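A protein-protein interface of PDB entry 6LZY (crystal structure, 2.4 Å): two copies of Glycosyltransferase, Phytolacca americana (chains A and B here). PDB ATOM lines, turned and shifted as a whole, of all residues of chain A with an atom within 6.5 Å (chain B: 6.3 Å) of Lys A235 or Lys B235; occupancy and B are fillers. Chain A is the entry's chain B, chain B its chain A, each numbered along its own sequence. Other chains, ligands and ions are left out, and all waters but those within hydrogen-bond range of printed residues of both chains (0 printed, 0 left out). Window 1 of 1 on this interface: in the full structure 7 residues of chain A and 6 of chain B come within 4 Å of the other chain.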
ATOM      1  N   THR A 151       3.043  -5.500 -18.783  1.00  0.00           N
ATOM      2  CA  THR A 151       2.588  -4.125 -19.135  1.00  0.00           C
ATOM      3  C   THR A 151       3.745  -3.146 -18.952  1.00  0.00           C
ATOM      4  O   THR A 151       4.054  -2.434 -19.918  1.00  0.00           O
ATOM      5  CB  THR A 151       1.379  -3.695 -18.310  1.00  0.00           C
ATOM      6  OG1 THR A 151       0.405  -4.722 -18.504  1.00  0.00           O
ATOM      7  CG2 THR A 151       0.859  -2.330 -18.711  1.00  0.00           C
ATOM      8  N   ARG A 161       0.694  -2.972 -24.495  1.00  0.00           N
ATOM      9  CA  ARG A 161       0.438  -4.368 -24.077  1.00  0.00           C
ATOM     10  C   ARG A 161      -1.073  -4.641 -24.032  1.00  0.00           C
ATOM     11  O   ARG A 161      -1.791  -3.874 -23.378  1.00  0.00           O
ATOM     12  CB  ARG A 161       1.053  -4.669 -22.710  1.00  0.00           C
ATOM     13  CG  ARG A 161       0.907  -6.129 -22.297  1.00  0.00           C
ATOM     14  CD  ARG A 161      -0.237  -6.365 -21.307  1.00  0.00           C
ATOM     15  NE  ARG A 161      -0.547  -7.764 -21.016  1.00  0.00           N
ATOM     16  CZ  ARG A 161      -0.369  -8.370 -19.834  1.00  0.00           C
ATOM     17  NH1 ARG A 161      -0.709  -9.634 -19.661  1.00  0.00           N
ATOM     18  NH2 ARG A 161       0.156  -7.722 -18.820  1.00  0.00           N
ATOM     19  N   LYS A 230      -6.306  -8.762 -12.536  1.00  0.00           N
ATOM     20  CA  LYS A 230      -7.516  -7.965 -12.856  1.00  0.00           C
ATOM     21  C   LYS A 230      -7.117  -6.495 -13.011  1.00  0.00           C
ATOM     22  O   LYS A 230      -7.600  -5.845 -13.937  1.00  0.00           O
ATOM     23  CB  LYS A 230      -8.629  -8.195 -11.837  1.00  0.00           C
ATOM     24  CG  LYS A 230      -9.049  -9.653 -11.633  1.00  0.00           C
ATOM     25  CD  LYS A 230      -9.594 -10.392 -12.860  1.00  0.00           C
ATOM     26  CE  LYS A 230     -10.856  -9.739 -13.379  1.00  0.00           C
ATOM     27  NZ  LYS A 230     -11.181 -10.181 -14.749  1.00  0.00           N
ATOM     28  N   GLU A 231      -6.181  -6.019 -12.203  1.00  0.00           N
ATOM     29  CA  GLU A 231      -5.659  -4.634 -12.317  1.00  0.00           C
ATOM     30  C   GLU A 231      -4.964  -4.452 -13.665  1.00  0.00           C
ATOM     31  O   GLU A 231      -5.080  -3.357 -14.210  1.00  0.00           O
ATOM     32  CB  GLU A 231      -4.747  -4.285 -11.136  1.00  0.00           C
ATOM     33  CG  GLU A 231      -5.505  -4.137  -9.822  1.00  0.00           C
ATOM     34  CD  GLU A 231      -4.740  -3.503  -8.665  1.00  0.00           C
ATOM     35  OE1 GLU A 231      -5.408  -2.966  -7.742  1.00  0.00           O
ATOM     36  OE2 GLU A 231      -3.489  -3.535  -8.680  1.00  0.00           O
ATOM     37  N   SER A 232      -4.289  -5.469 -14.197  1.00  0.00           N
ATOM     38  CA  SER A 232      -3.582  -5.352 -15.494  1.00  0.00           C
ATOM     39  C   SER A 232      -4.574  -4.984 -16.597  1.00  0.00           C
ATOM     40  O   SER A 232      -4.148  -4.449 -17.605  1.00  0.00           O
ATOM     41  CB  SER A 232      -2.831  -6.622 -15.826  1.00  0.00           C
ATOM     42  OG  SER A 232      -3.703  -7.653 -16.273  1.00  0.00           O
ATOM     43  N   GLU A 233      -5.843  -5.339 -16.442  1.00  0.00           N
ATOM     44  CA  GLU A 233      -6.866  -5.121 -17.494  1.00  0.00           C
ATOM     45  C   GLU A 233      -7.075  -3.619 -17.688  1.00  0.00           C
ATOM     46  O   GLU A 233      -7.348  -3.225 -18.837  1.00  0.00           O
ATOM     47  CB  GLU A 233      -8.200  -5.808 -17.166  1.00  0.00           C
ATOM     48  CG  GLU A 233      -8.115  -7.326 -17.154  1.00  0.00           C
ATOM     49  CD  GLU A 233      -9.267  -8.039 -16.455  1.00  0.00           C
ATOM     50  OE1 GLU A 233     -10.273  -7.392 -16.187  1.00  0.00           O
ATOM     51  OE2 GLU A 233      -9.146  -9.248 -16.188  1.00  0.00           O
ATOM     52  N   LEU A 234      -6.974  -2.826 -16.617  1.00  0.00           N
ATOM     53  CA  LEU A 234      -7.143  -1.344 -16.691  1.00  0.00           C
ATOM     54  C   LEU A 234      -5.786  -0.668 -16.928  1.00  0.00           C
ATOM     55  O   LEU A 234      -5.754   0.364 -17.600  1.00  0.00           O
ATOM     56  CB  LEU A 234      -7.788  -0.858 -15.390  1.00  0.00           C
ATOM     57  CG  LEU A 234      -9.268  -1.196 -15.217  1.00  0.00           C
ATOM     58  CD1 LEU A 234      -9.806  -0.720 -13.883  1.00  0.00           C
ATOM     59  CD2 LEU A 234     -10.079  -0.599 -16.342  1.00  0.00           C
ATOM     60  N   LYS A 235      -4.694  -1.230 -16.406  1.00  0.00           N
ATOM     61  CA  LYS A 235      -3.347  -0.580 -16.476  1.00  0.00           C
ATOM     62  C   LYS A 235      -2.765  -0.717 -17.890  1.00  0.00           C
ATOM     63  O   LYS A 235      -1.908   0.115 -18.263  1.00  0.00           O
ATOM     64  CB  LYS A 235      -2.391  -1.252 -15.482  1.00  0.00           C
ATOM     65  CG  LYS A 235      -1.931  -0.400 -14.306  1.00  0.00           C
ATOM     66  CD  LYS A 235      -2.635  -0.681 -13.013  1.00  0.00           C
ATOM     67  CE  LYS A 235      -2.404   0.431 -12.020  1.00  0.00           C
ATOM     68  NZ  LYS A 235      -3.007   0.094 -10.717  1.00  0.00           N
ATOM     69  N   SER A 236      -3.180  -1.746 -18.634  1.00  0.00           N
ATOM     70  CA  SER A 236      -2.622  -2.090 -19.965  1.00  0.00           C
ATOM     71  C   SER A 236      -3.353  -1.284 -21.029  1.00  0.00           C
ATOM     72  O   SER A 236      -4.299  -0.563 -20.699  1.00  0.00           O
ATOM     73  CB  SER A 236      -2.737  -3.581 -20.231  1.00  0.00           C
ATOM     74  OG  SER A 236      -2.128  -4.346 -19.195  1.00  0.00           O
ATOM     75  N   TYR A 237      -2.992  -1.457 -22.295  1.00  0.00           N
ATOM     76  CA  TYR A 237      -3.681  -0.768 -23.410  1.00  0.00           C
ATOM     77  C   TYR A 237      -5.111  -1.332 -23.558  1.00  0.00           C
ATOM     78  O   TYR A 237      -6.017  -0.570 -23.929  1.00  0.00           O
ATOM     79  CB  TYR A 237      -2.882  -0.865 -24.705  1.00  0.00           C
ATOM     80  CG  TYR A 237      -3.411   0.006 -25.812  1.00  0.00           C
ATOM     81  CD1 TYR A 237      -3.262   1.392 -25.773  1.00  0.00           C
ATOM     82  CD2 TYR A 237      -4.058  -0.546 -26.909  1.00  0.00           C
ATOM     83  CE1 TYR A 237      -3.768   2.201 -26.787  1.00  0.00           C
ATOM     84  CE2 TYR A 237      -4.579   0.247 -27.917  1.00  0.00           C
ATOM     85  CZ  TYR A 237      -4.419   1.618 -27.867  1.00  0.00           C
ATOM     86  OH  TYR A 237      -4.924   2.391 -28.872  1.00  0.00           O
ATOM     87  N   GLY A 238      -5.306  -2.603 -23.254  1.00  0.00           N
ATOM     88  CA  GLY A 238      -6.624  -3.229 -23.289  1.00  0.00           C
ATOM     89  C   GLY A 238      -6.570  -4.736 -23.329  1.00  0.00           C
ATOM     90  O   GLY A 238      -5.511  -5.315 -23.052  1.00  0.00           O
ATOM     91  N   THR B 151       3.269   8.973 -16.373  1.00  0.00           N
ATOM     92  CA  THR B 151       3.155   7.621 -15.769  1.00  0.00           C
ATOM     93  C   THR B 151       4.233   6.710 -16.354  1.00  0.00           C
ATOM     94  O   THR B 151       4.997   6.118 -15.577  1.00  0.00           O
ATOM     95  CB  THR B 151       1.758   7.047 -15.952  1.00  0.00           C
ATOM     96  OG1 THR B 151       0.846   8.054 -15.504  1.00  0.00           O
ATOM     97  CG2 THR B 151       1.606   5.755 -15.178  1.00  0.00           C
ATOM     98  N   LYS B 230      -8.109  11.352 -18.147  1.00  0.00           N
ATOM     99  CA  LYS B 230      -9.020  10.502 -17.323  1.00  0.00           C
ATOM    100  C   LYS B 230      -8.448   9.085 -17.281  1.00  0.00           C
ATOM    101  O   LYS B 230      -8.446   8.474 -16.207  1.00  0.00           O
ATOM    102  CB  LYS B 230     -10.438  10.569 -17.889  1.00  0.00           C
ATOM    103  CG  LYS B 230     -11.032  11.973 -17.834  1.00  0.00           C
ATOM    104  CD  LYS B 230     -11.760  12.233 -16.541  1.00  0.00           C
ATOM    105  CE  LYS B 230     -11.038  13.074 -15.517  1.00  0.00           C
ATOM    106  NZ  LYS B 230     -11.599  12.803 -14.165  1.00  0.00           N
ATOM    107  N   GLU B 231      -7.915   8.603 -18.394  1.00  0.00           N
ATOM    108  CA  GLU B 231      -7.283   7.262 -18.452  1.00  0.00           C
ATOM    109  C   GLU B 231      -6.071   7.216 -17.513  1.00  0.00           C
ATOM    110  O   GLU B 231      -5.839   6.165 -16.926  1.00  0.00           O
ATOM    111  CB  GLU B 231      -6.930   6.891 -19.893  1.00  0.00           C
ATOM    112  CG  GLU B 231      -8.143   6.624 -20.787  1.00  0.00           C
ATOM    113  CD  GLU B 231      -7.775   6.157 -22.194  1.00  0.00           C
ATOM    114  OE1 GLU B 231      -6.568   6.180 -22.508  1.00  0.00           O
ATOM    115  OE2 GLU B 231      -8.672   5.758 -22.972  1.00  0.00           O
ATOM    116  N   SER B 232      -5.318   8.301 -17.370  1.00  0.00           N
ATOM    117  CA  SER B 232      -4.122   8.313 -16.501  1.00  0.00           C
ATOM    118  C   SER B 232      -4.518   7.992 -15.052  1.00  0.00           C
ATOM    119  O   SER B 232      -3.679   7.561 -14.292  1.00  0.00           O
ATOM    120  CB  SER B 232      -3.377   9.630 -16.605  1.00  0.00           C
ATOM    121  OG  SER B 232      -4.013  10.653 -15.879  1.00  0.00           O
ATOM    122  N   GLU B 233      -5.752   8.268 -14.672  1.00  0.00           N
ATOM    123  CA  GLU B 233      -6.223   8.067 -13.277  1.00  0.00           C
ATOM    124  C   GLU B 233      -6.216   6.569 -12.945  1.00  0.00           C
ATOM    125  O   GLU B 233      -5.973   6.247 -11.785  1.00  0.00           O
ATOM    126  CB  GLU B 233      -7.624   8.654 -13.079  1.00  0.00           C
ATOM    127  CG  GLU B 233      -7.671  10.153 -13.139  1.00  0.00           C
ATOM    128  CD  GLU B 233      -9.036  10.807 -13.356  1.00  0.00           C
ATOM    129  OE1 GLU B 233     -10.074  10.143 -13.183  1.00  0.00           O
ATOM    130  OE2 GLU B 233      -9.037  12.009 -13.695  1.00  0.00           O
ATOM    131  N   LEU B 234      -6.506   5.702 -13.919  1.00  0.00           N
ATOM    132  CA  LEU B 234      -6.500   4.227 -13.713  1.00  0.00           C
ATOM    133  C   LEU B 234      -5.116   3.650 -14.047  1.00  0.00           C
ATOM    134  O   LEU B 234      -4.713   2.673 -13.389  1.00  0.00           O
ATOM    135  CB  LEU B 234      -7.598   3.593 -14.578  1.00  0.00           C
ATOM    136  CG  LEU B 234      -9.035   3.866 -14.121  1.00  0.00           C
ATOM    137  CD1 LEU B 234     -10.037   3.252 -15.086  1.00  0.00           C
ATOM    138  CD2 LEU B 234      -9.269   3.373 -12.700  1.00  0.00           C
ATOM    139  N   LYS B 235      -4.393   4.234 -15.008  1.00  0.00           N
ATOM    140  CA  LYS B 235      -3.089   3.665 -15.467  1.00  0.00           C
ATOM    141  C   LYS B 235      -1.982   3.951 -14.444  1.00  0.00           C
ATOM    142  O   LYS B 235      -0.981   3.210 -14.420  1.00  0.00           O
ATOM    143  CB  LYS B 235      -2.635   4.255 -16.802  1.00  0.00           C
ATOM    144  CG  LYS B 235      -3.690   4.278 -17.883  1.00  0.00           C
ATOM    145  CD  LYS B 235      -3.607   3.188 -18.905  1.00  0.00           C
ATOM    146  CE  LYS B 235      -4.364   3.576 -20.154  1.00  0.00           C
ATOM    147  NZ  LYS B 235      -4.497   2.441 -21.090  1.00  0.00           N
ATOM    148  N   SER B 236      -2.134   5.004 -13.651  1.00  0.00           N
ATOM    149  CA  SER B 236      -1.106   5.493 -12.690  1.00  0.00           C
ATOM    150  C   SER B 236      -1.262   4.736 -11.379  1.00  0.00           C
ATOM    151  O   SER B 236      -2.197   3.951 -11.245  1.00  0.00           O
ATOM    152  CB  SER B 236      -1.230   6.995 -12.494  1.00  0.00           C
ATOM    153  OG  SER B 236      -1.155   7.676 -13.747  1.00  0.00           O
ATOM    154  N   TYR B 237      -0.414   5.007 -10.400  1.00  0.00           N
ATOM    155  CA  TYR B 237      -0.509   4.351  -9.080  1.00  0.00           C
ATOM    156  C   TYR B 237      -1.761   4.849  -8.352  1.00  0.00           C
ATOM    157  O   TYR B 237      -2.376   4.077  -7.591  1.00  0.00           O
ATOM    158  CB  TYR B 237       0.757   4.586  -8.269  1.00  0.00           C
ATOM    159  CG  TYR B 237       0.835   3.758  -7.016  1.00  0.00           C
ATOM    160  CD1 TYR B 237       1.074   2.395  -7.083  1.00  0.00           C
ATOM    161  CD2 TYR B 237       0.680   4.338  -5.771  1.00  0.00           C
ATOM    162  CE1 TYR B 237       1.151   1.624  -5.937  1.00  0.00           C
ATOM    163  CE2 TYR B 237       0.750   3.582  -4.614  1.00  0.00           C
ATOM    164  CZ  TYR B 237       0.984   2.218  -4.698  1.00  0.00           C
ATOM    165  OH  TYR B 237       1.054   1.462  -3.562  1.00  0.00           O
ATOM    166  N   GLY B 238      -2.153   6.097  -8.584  1.00  0.00           N
ATOM    167  CA  GLY B 238      -3.378   6.648  -7.985  1.00  0.00           C
ATOM    168  C   GLY B 238      -3.415   8.156  -8.045  1.00  0.00           C
ATOM    169  O   GLY B 238      -2.600   8.750  -8.770  1.00  0.00           O
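Lys B235 touches three residues of chain A. Of the printed residues of chain A, Ser B236 touches Lys A235 (3.6 Å). Printed residues of chain B within 4 Å of Ser A236: Lys B235. Gly A238 touches none of the printed residues of chain B. Lys A230 touches none of the printed residues of chain B.
Leu A234 touches Lys B235, and with the chains exchanged Lys A235 touches Leu B234. Lys A235 touches its own counterpart, Lys B235. Lys A235 touches Ser B236, and with the chains exchanged Ser A236 touches Lys B235. 10 positions are printed for both chains. Of the 5 pairs that touch across the chains among the printed residues, 5 have their exchanged pair printed and touching as well.
OG1 of Thr B151 sits at hydrogen-bond distance from OG of Ser B236 (2.7 Å). O of Ser B232 sits at hydrogen-bond distance from OG of Ser B236. The side-chain hydroxyl (OG1) of Thr A151 is in hydrogen-bond range of the side-chain hydroxyl (OG) of Ser A236 (2.7 Å). O of Ser A232 sits at hydrogen-bond distance from OG of Ser A236 (2.6 Å).
Leu A234 touches Lys B235. Lys A235 touches Leu B234 (CE to O, 3.5 Å). O of Lys A235 touches CD of Lys B235, at 3.6 Å. Ser B236 touches Lys A235.
The backbone carbonyl oxygen (O) of Ser A236 is in hydrogen-bond range of the side-chain amino group (NZ) of Lys B235 (3.0 Å).
Printed residues of chain A that touch a printed residue of chain B: Leu A234, Lys A235 and Ser A236. Among the printed residues, no Asp or Glu carboxylate lies within 4 Å of a Lys or Arg side-chain nitrogen of the other chain.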
